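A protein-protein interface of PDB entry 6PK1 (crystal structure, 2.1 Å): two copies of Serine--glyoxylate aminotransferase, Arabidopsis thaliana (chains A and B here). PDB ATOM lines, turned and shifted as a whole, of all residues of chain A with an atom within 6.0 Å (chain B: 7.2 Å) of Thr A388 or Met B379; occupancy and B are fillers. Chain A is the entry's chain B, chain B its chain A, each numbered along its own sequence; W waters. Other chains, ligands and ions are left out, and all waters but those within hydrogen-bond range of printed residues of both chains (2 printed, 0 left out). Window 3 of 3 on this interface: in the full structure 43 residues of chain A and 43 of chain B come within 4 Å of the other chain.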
ATOM      1  N   GLY A 380      14.001  -8.720   5.664  1.00  0.00           N
ATOM      2  CA  GLY A 380      14.205  -7.317   5.897  1.00  0.00           C
ATOM      3  C   GLY A 380      12.954  -6.470   5.853  1.00  0.00           C
ATOM      4  O   GLY A 380      12.990  -5.338   6.335  1.00  0.00           O
ATOM      5  N   VAL A 383      11.573  -5.727   9.539  1.00  0.00           N
ATOM      6  CA  VAL A 383      12.601  -4.926  10.188  1.00  0.00           C
ATOM      7  C   VAL A 383      12.604  -3.517   9.613  1.00  0.00           C
ATOM      8  O   VAL A 383      12.635  -2.526  10.352  1.00  0.00           O
ATOM      9  CB  VAL A 383      13.977  -5.593  10.007  1.00  0.00           C
ATOM     10  CG1 VAL A 383      15.068  -4.680  10.534  1.00  0.00           C
ATOM     11  CG2 VAL A 383      14.020  -6.971  10.663  1.00  0.00           C
ATOM     12  N   ALA A 384      12.549  -3.411   8.279  1.00  0.00           N
ATOM     13  CA  ALA A 384      12.574  -2.112   7.630  1.00  0.00           C
ATOM     14  C   ALA A 384      11.373  -1.261   8.015  1.00  0.00           C
ATOM     15  O   ALA A 384      11.504  -0.043   8.152  1.00  0.00           O
ATOM     16  CB  ALA A 384      12.617  -2.280   6.100  1.00  0.00           C
ATOM     17  N   ALA A 385      10.180  -1.863   8.129  1.00  0.00           N
ATOM     18  CA  ALA A 385       9.010  -1.083   8.524  1.00  0.00           C
ATOM     19  C   ALA A 385       9.131  -0.594   9.961  1.00  0.00           C
ATOM     20  O   ALA A 385       8.805   0.568  10.271  1.00  0.00           O
ATOM     21  CB  ALA A 385       7.751  -1.909   8.384  1.00  0.00           C
ATOM     22  N   ALA A 386       9.583  -1.479  10.852  1.00  0.00           N
ATOM     23  CA  ALA A 386       9.738  -1.121  12.260  1.00  0.00           C
ATOM     24  C   ALA A 386      10.811  -0.035  12.438  1.00  0.00           C
ATOM     25  O   ALA A 386      10.610   0.957  13.179  1.00  0.00           O
ATOM     26  CB  ALA A 386      10.089  -2.377  13.053  1.00  0.00           C
ATOM     27  N   SER A 387      11.923  -0.176  11.708  1.00  0.00           N
ATOM     28  CA  SER A 387      13.048   0.740  11.856  1.00  0.00           C
ATOM     29  C   SER A 387      12.695   2.099  11.288  1.00  0.00           C
ATOM     30  O   SER A 387      13.156   3.115  11.786  1.00  0.00           O
ATOM     31  CB  SER A 387      14.279   0.200  11.122  1.00  0.00           C
ATOM     32  OG  SER A 387      14.720  -0.949  11.729  1.00  0.00           O
ATOM     33  N   THR A 388      11.964   2.128  10.170  1.00  0.00           N
ATOM     34  CA  THR A 388      11.572   3.401   9.610  1.00  0.00           C
ATOM     35  C   THR A 388      10.726   4.142  10.608  1.00  0.00           C
ATOM     36  O   THR A 388      10.841   5.357  10.769  1.00  0.00           O
ATOM     37  CB  THR A 388      10.809   3.164   8.294  1.00  0.00           C
ATOM     38  OG1 THR A 388      11.655   2.512   7.346  1.00  0.00           O
ATOM     39  CG2 THR A 388      10.308   4.472   7.729  1.00  0.00           C
ATOM     40  N   TYR A 389       9.809   3.441  11.246  1.00  0.00           N
ATOM     41  CA  TYR A 389       8.989   4.110  12.248  1.00  0.00           C
ATOM     42  C   TYR A 389       9.837   4.531  13.438  1.00  0.00           C
ATOM     43  O   TYR A 389       9.757   5.669  13.902  1.00  0.00           O
ATOM     44  CB  TYR A 389       7.860   3.178  12.684  1.00  0.00           C
ATOM     45  CG  TYR A 389       7.186   3.590  13.963  1.00  0.00           C
ATOM     46  CD1 TYR A 389       6.225   4.624  13.984  1.00  0.00           C
ATOM     47  CD2 TYR A 389       7.474   2.957  15.127  1.00  0.00           C
ATOM     48  CE1 TYR A 389       5.577   4.967  15.177  1.00  0.00           C
ATOM     49  CE2 TYR A 389       6.840   3.301  16.314  1.00  0.00           C
ATOM     50  CZ  TYR A 389       5.931   4.290  16.340  1.00  0.00           C
ATOM     51  OH  TYR A 389       5.353   4.596  17.512  1.00  0.00           O
ATOM     52  N   LEU A 390      10.665   3.621  13.951  1.00  0.00           N
ATOM     53  CA  LEU A 390      11.373   3.920  15.207  1.00  0.00           C
ATOM     54  C   LEU A 390      12.398   5.018  15.051  1.00  0.00           C
ATOM     55  O   LEU A 390      12.623   5.782  15.983  1.00  0.00           O
ATOM     56  CB  LEU A 390      12.060   2.684  15.730  1.00  0.00           C
ATOM     57  CG  LEU A 390      11.120   1.609  16.296  1.00  0.00           C
ATOM     58  CD1 LEU A 390      11.919   0.369  16.560  1.00  0.00           C
ATOM     59  CD2 LEU A 390      10.429   2.042  17.502  1.00  0.00           C
ATOM     60  N   GLN A 391      13.040   5.121  13.892  1.00  0.00           N
ATOM     61  CA  GLN A 391      14.015   6.175  13.670  1.00  0.00           C
ATOM     62  C   GLN A 391      13.417   7.551  13.831  1.00  0.00           C
ATOM     63  O   GLN A 391      14.173   8.506  14.079  1.00  0.00           O
ATOM     64  CB  GLN A 391      14.626   6.015  12.258  1.00  0.00           C
ATOM     65  CG  GLN A 391      15.738   7.007  11.913  1.00  0.00           C
ATOM     66  CD  GLN A 391      15.223   8.327  11.328  1.00  0.00           C
ATOM     67  OE1 GLN A 391      14.096   8.392  10.888  1.00  0.00           O
ATOM     68  NE2 GLN A 391      16.057   9.393  11.366  1.00  0.00           N
ATOM     69  N   HIS A 392      12.090   7.693  13.710  1.00  0.00           N
ATOM     70  CA  HIS A 392      11.468   8.998  13.906  1.00  0.00           C
ATOM     71  C   HIS A 392      11.063   9.253  15.351  1.00  0.00           C
ATOM     72  O   HIS A 392      10.909  10.416  15.748  1.00  0.00           O
ATOM     73  CB  HIS A 392      10.223   9.127  13.022  1.00  0.00           C
ATOM     74  CG  HIS A 392       9.581  10.474  13.060  1.00  0.00           C
ATOM     75  ND1 HIS A 392       9.872  11.460  12.144  1.00  0.00           N
ATOM     76  CD2 HIS A 392       8.658  10.997  13.898  1.00  0.00           C
ATOM     77  CE1 HIS A 392       9.159  12.535  12.424  1.00  0.00           C
ATOM     78  NE2 HIS A 392       8.416  12.281  13.484  1.00  0.00           N
ATOM     79  N   ALA B 364      20.674  -3.485  12.723  1.00  0.00           N
ATOM     80  CA  ALA B 364      19.480  -2.677  12.477  1.00  0.00           C
ATOM     81  C   ALA B 364      19.623  -1.289  13.090  1.00  0.00           C
ATOM     82  O   ALA B 364      19.185  -0.267  12.498  1.00  0.00           O
ATOM     83  CB  ALA B 364      18.246  -3.356  13.042  1.00  0.00           C
ATOM     84  N   VAL B 366      22.452   0.295  13.412  1.00  0.00           N
ATOM     85  CA  VAL B 366      23.389   1.046  12.579  1.00  0.00           C
ATOM     86  C   VAL B 366      22.674   1.680  11.386  1.00  0.00           C
ATOM     87  O   VAL B 366      22.946   2.835  11.036  1.00  0.00           O
ATOM     88  CB  VAL B 366      24.560   0.153  12.140  1.00  0.00           C
ATOM     89  CG1 VAL B 366      25.381   0.876  11.089  1.00  0.00           C
ATOM     90  CG2 VAL B 366      25.454  -0.183  13.399  1.00  0.00           C
ATOM     91  N   GLU B 367      21.696   0.973  10.800  1.00  0.00           N
ATOM     92  CA  GLU B 367      20.927   1.556   9.715  1.00  0.00           C
ATOM     93  C   GLU B 367      20.203   2.816  10.157  1.00  0.00           C
ATOM     94  O   GLU B 367      20.154   3.788   9.397  1.00  0.00           O
ATOM     95  CB  GLU B 367      19.959   0.513   9.148  1.00  0.00           C
ATOM     96  CG  GLU B 367      20.698  -0.670   8.480  1.00  0.00           C
ATOM     97  CD  GLU B 367      19.809  -1.713   7.805  1.00  0.00           C
ATOM     98  OE1 GLU B 367      18.557  -1.644   7.933  1.00  0.00           O
ATOM     99  OE2 GLU B 367      20.398  -2.580   7.121  1.00  0.00           O
ATOM    100  N   MET B 368      19.636   2.822  11.376  1.00  0.00           N
ATOM    101  CA  MET B 368      18.934   4.011  11.839  1.00  0.00           C
ATOM    102  C   MET B 368      19.920   5.142  12.077  1.00  0.00           C
ATOM    103  O   MET B 368      19.626   6.304  11.792  1.00  0.00           O
ATOM    104  CB  MET B 368      18.143   3.720  13.135  1.00  0.00           C
ATOM    105  CG  MET B 368      16.940   2.797  12.862  1.00  0.00           C
ATOM    106  SD  MET B 368      15.875   2.557  14.238  1.00  0.00           S
ATOM    107  CE  MET B 368      16.936   1.470  15.211  1.00  0.00           C
ATOM    108  N   ILE B 369      21.086   4.832  12.640  1.00  0.00           N
ATOM    109  CA  ILE B 369      22.098   5.875  12.867  1.00  0.00           C
ATOM    110  C   ILE B 369      22.535   6.483  11.545  1.00  0.00           C
ATOM    111  O   ILE B 369      22.714   7.695  11.421  1.00  0.00           O
ATOM    112  CB  ILE B 369      23.292   5.287  13.623  1.00  0.00           C
ATOM    113  CG1 ILE B 369      22.858   4.821  15.026  1.00  0.00           C
ATOM    114  CG2 ILE B 369      24.419   6.325  13.684  1.00  0.00           C
ATOM    115  CD1 ILE B 369      23.784   3.728  15.586  1.00  0.00           C
ATOM    116  N   LEU B 370      22.767   5.639  10.550  1.00  0.00           N
ATOM    117  CA  LEU B 370      23.189   6.142   9.255  1.00  0.00           C
ATOM    118  C   LEU B 370      22.167   7.121   8.707  1.00  0.00           C
ATOM    119  O   LEU B 370      22.520   8.170   8.154  1.00  0.00           O
ATOM    120  CB  LEU B 370      23.380   4.967   8.292  1.00  0.00           C
ATOM    121  CG  LEU B 370      24.668   4.148   8.478  1.00  0.00           C
ATOM    122  CD1 LEU B 370      24.681   2.925   7.625  1.00  0.00           C
ATOM    123  CD2 LEU B 370      25.899   5.051   8.156  1.00  0.00           C
ATOM    124  N   LYS B 371      20.893   6.789   8.824  1.00  0.00           N
ATOM    125  CA  LYS B 371      19.886   7.749   8.392  1.00  0.00           C
ATOM    126  C   LYS B 371      19.984   9.043   9.210  1.00  0.00           C
ATOM    127  O   LYS B 371      19.922  10.161   8.655  1.00  0.00           O
ATOM    128  CB  LYS B 371      18.498   7.120   8.498  1.00  0.00           C
ATOM    129  CG  LYS B 371      17.406   8.152   8.303  1.00  0.00           C
ATOM    130  CD  LYS B 371      16.292   7.659   7.441  1.00  0.00           C
ATOM    131  CE  LYS B 371      15.383   8.856   7.097  1.00  0.00           C
ATOM    132  NZ  LYS B 371      14.054   8.427   6.632  1.00  0.00           N
ATOM    133  N   ASP B 372      20.156   8.900  10.531  1.00  0.00           N
ATOM    134  CA  ASP B 372      20.230  10.066  11.406  1.00  0.00           C
ATOM    135  C   ASP B 372      21.289  11.052  10.954  1.00  0.00           C
ATOM    136  O   ASP B 372      21.111  12.265  11.130  1.00  0.00           O
ATOM    137  CB  ASP B 372      20.563   9.658  12.860  1.00  0.00           C
ATOM    138  CG  ASP B 372      19.373   9.130  13.622  1.00  0.00           C
ATOM    139  OD1 ASP B 372      18.216   9.282  13.186  1.00  0.00           O
ATOM    140  OD2 ASP B 372      19.598   8.546  14.689  1.00  0.00           O
ATOM    141  N   TYR B 375      23.120   9.735   5.753  1.00  0.00           N
ATOM    142  CA  TYR B 375      23.601   8.812   4.764  1.00  0.00           C
ATOM    143  C   TYR B 375      22.414   8.052   4.175  1.00  0.00           C
ATOM    144  O   TYR B 375      21.636   7.500   4.919  1.00  0.00           O
ATOM    145  CB  TYR B 375      24.604   7.832   5.358  1.00  0.00           C
ATOM    146  CG  TYR B 375      25.175   6.862   4.315  1.00  0.00           C
ATOM    147  CD1 TYR B 375      26.127   7.277   3.395  1.00  0.00           C
ATOM    148  CD2 TYR B 375      24.723   5.546   4.232  1.00  0.00           C
ATOM    149  CE1 TYR B 375      26.636   6.389   2.396  1.00  0.00           C
ATOM    150  CE2 TYR B 375      25.214   4.664   3.278  1.00  0.00           C
ATOM    151  CZ  TYR B 375      26.182   5.089   2.372  1.00  0.00           C
ATOM    152  OH  TYR B 375      26.695   4.209   1.434  1.00  0.00           O
ATOM    153  N   PRO B 376      22.267   7.961   2.856  1.00  0.00           N
ATOM    154  CA  PRO B 376      21.038   7.369   2.288  1.00  0.00           C
ATOM    155  C   PRO B 376      21.077   5.846   2.211  1.00  0.00           C
ATOM    156  O   PRO B 376      21.204   5.235   1.132  1.00  0.00           O
ATOM    157  CB  PRO B 376      20.968   8.037   0.900  1.00  0.00           C
ATOM    158  CG  PRO B 376      22.400   8.246   0.507  1.00  0.00           C
ATOM    159  CD  PRO B 376      23.177   8.462   1.798  1.00  0.00           C
ATOM    160  N   VAL B 377      20.922   5.196   3.354  1.00  0.00           N
ATOM    161  CA  VAL B 377      20.786   3.747   3.392  1.00  0.00           C
ATOM    162  C   VAL B 377      19.351   3.337   3.064  1.00  0.00           C
ATOM    163  O   VAL B 377      18.400   4.044   3.360  1.00  0.00           O
ATOM    164  CB  VAL B 377      21.214   3.248   4.784  1.00  0.00           C
ATOM    165  CG1 VAL B 377      20.292   3.858   5.857  1.00  0.00           C
ATOM    166  CG2 VAL B 377      21.164   1.728   4.859  1.00  0.00           C
ATOM    167  N   VAL B 378      19.172   2.199   2.407  1.00  0.00           N
ATOM    168  CA  VAL B 378      17.846   1.606   2.230  1.00  0.00           C
ATOM    169  C   VAL B 378      17.559   0.751   3.479  1.00  0.00           C
ATOM    170  O   VAL B 378      18.274  -0.218   3.786  1.00  0.00           O
ATOM    171  CB  VAL B 378      17.773   0.754   0.963  1.00  0.00           C
ATOM    172  CG1 VAL B 378      16.375   0.184   0.789  1.00  0.00           C
ATOM    173  CG2 VAL B 378      18.088   1.593  -0.255  1.00  0.00           C
ATOM    174  N   MET B 379      16.547   1.147   4.242  1.00  0.00           N
ATOM    175  CA  MET B 379      16.235   0.510   5.515  1.00  0.00           C
ATOM    176  C   MET B 379      15.986  -0.975   5.274  1.00  0.00           C
ATOM    177  O   MET B 379      15.247  -1.366   4.353  1.00  0.00           O
ATOM    178  CB  MET B 379      15.007   1.195   6.114  1.00  0.00           C
ATOM    179  CG  MET B 379      14.993   1.285   7.626  1.00  0.00           C
ATOM    180  SD  MET B 379      16.463   2.032   8.416  1.00  0.00           S
ATOM    181  CE  MET B 379      16.527   3.581   7.854  1.00  0.00           C
ATOM    182  N   GLY B 380      16.664  -1.791   6.051  1.00  0.00           N
ATOM    183  CA  GLY B 380      16.527  -3.224   5.984  1.00  0.00           C
ATOM    184  C   GLY B 380      17.505  -3.928   5.071  1.00  0.00           C
ATOM    185  O   GLY B 380      17.620  -5.150   5.140  1.00  0.00           O
ATOM    186  N   SER B 381      18.224  -3.195   4.235  1.00  0.00           N
ATOM    187  CA  SER B 381      19.025  -3.831   3.202  1.00  0.00           C
ATOM    188  C   SER B 381      20.205  -4.600   3.789  1.00  0.00           C
ATOM    189  O   SER B 381      20.513  -5.698   3.326  1.00  0.00           O
ATOM    190  CB  SER B 381      19.505  -2.780   2.187  1.00  0.00           C
ATOM    191  OG  SER B 381      20.313  -1.821   2.866  1.00  0.00           O
ATOM    192  N   GLY B 382      20.876  -4.054   4.793  1.00  0.00           N
ATOM    193  CA  GLY B 382      21.953  -4.769   5.451  1.00  0.00           C
ATOM    194  C   GLY B 382      21.472  -5.889   6.379  1.00  0.00           C
ATOM    195  O   GLY B 382      22.047  -6.998   6.409  1.00  0.00           O
ATOM    196  N   VAL B 383      20.435  -5.608   7.167  1.00  0.00           N
ATOM    197  CA  VAL B 383      19.844  -6.665   7.965  1.00  0.00           C
ATOM    198  C   VAL B 383      19.436  -7.826   7.082  1.00  0.00           C
ATOM    199  O   VAL B 383      19.757  -8.980   7.386  1.00  0.00           O
ATOM    200  CB  VAL B 383      18.648  -6.145   8.778  1.00  0.00           C
ATOM    201  CG1 VAL B 383      17.989  -7.303   9.539  1.00  0.00           C
ATOM    202  CG2 VAL B 383      19.110  -5.088   9.750  1.00  0.00           C
ATOM    203  N   ALA B 384      18.806  -7.529   5.939  1.00  0.00           N
ATOM    204  CA  ALA B 384      18.326  -8.580   5.047  1.00  0.00           C
ATOM    205  C   ALA B 384      19.473  -9.382   4.444  1.00  0.00           C
ATOM    206  O   ALA B 384      19.365 -10.607   4.289  1.00  0.00           O
ATOM    207  CB  ALA B 384      17.493  -7.994   3.902  1.00  0.00           C
HETATM  208  O   HOH W   1      12.474   6.931   9.074  1.00  0.00           O
HETATM  209  O   HOH W   2      17.054  -1.433  10.325  1.00  0.00           O
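Among the printed residues, merely in contact across the chains: Ala A384 with Met B379, Thr A388 with Met B379, Gln A391 with Lys B371, Ser A387 with Met B379, Gln A391 with Met B368 and Gly A380 with Ala B384.
Gly A380 touches Ala B384, but with the chains exchanged Ala A384 does not touch Gly B380 (4.02 Å). 3 positions are printed for both chains.
The side-chain hydroxyl (OG) of Ser A387 sits at hydrogen-bond distance from the backbone carbonyl oxygen (O) of Val A383 (3.0 Å). O of Ala A384 sits at hydrogen-bond distance from OG1 of Thr A388 (2.7 Å).
Of the 18 printed residues of chain B, 5 touch a printed residue of chain A. Hydrophobic or aromatic side chains of chain B that line the printed part of chain A: Met B368, Met B379 and Ala B384. Printed residues of chain A that touch a printed residue of chain B: Gly A380, Ala A384, Ser A387, Thr A388 and Gln A391. Hydrophobic or aromatic side chains of chain A within 4 Å of the printed part of chain B: Ala A384. Along chain A the printed residues that touch a printed residue of chain B span positions 380 to 391. Among the printed residues, 8 pairs touch across the chains. Among the printed residues, no Asp or Glu carboxylate lies within 4 Å of a Lys or Arg side-chain nitrogen of the other chain.
Water W2 lies within hydrogen-bond range of the side-chain hydroxyl (OG) of Ser A387 (2.8 Å), the side-chain carboxylate (OE1) of Glu B367 (2.8 Å) and the backbone carbonyl oxygen (O) of Ala B364 (3.3 Å). Water W1 lies within hydrogen-bond range of the backbone carbonyl oxygen of Thr A388 (2.8 Å), the side-chain amide oxygen of Gln A391 (2.8 Å) and the side-chain amino group of Lys B371 (3.3 Å).
Printed residues of chain B within 4 Å of Gly A380: Ala B384. Of the printed residues of chain B, Ala A384 touches Met B379 (3.3 Å). Leu A390 touches none of the printed residues of chain B. Printed residues of chain A within 4 Å of Met B368: Ser A387 (3.7 Å) and Gln A391 (3.8 Å). Printed residues of chain A within 4 Å of Lys B371: Gln A391 (3.6 Å). Met B379 touches just these residues of chain A: Ala A384, Ser A387 and Thr A388.
NE2 of Gln A391 lies within hydrogen-bond range of OD1 of Asp B372 (2.8 Å). The backbone carbonyl oxygen (O) of Ser A387 lies close to the side-chain sulfur (SD) of Met B368 (3.7 Å).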
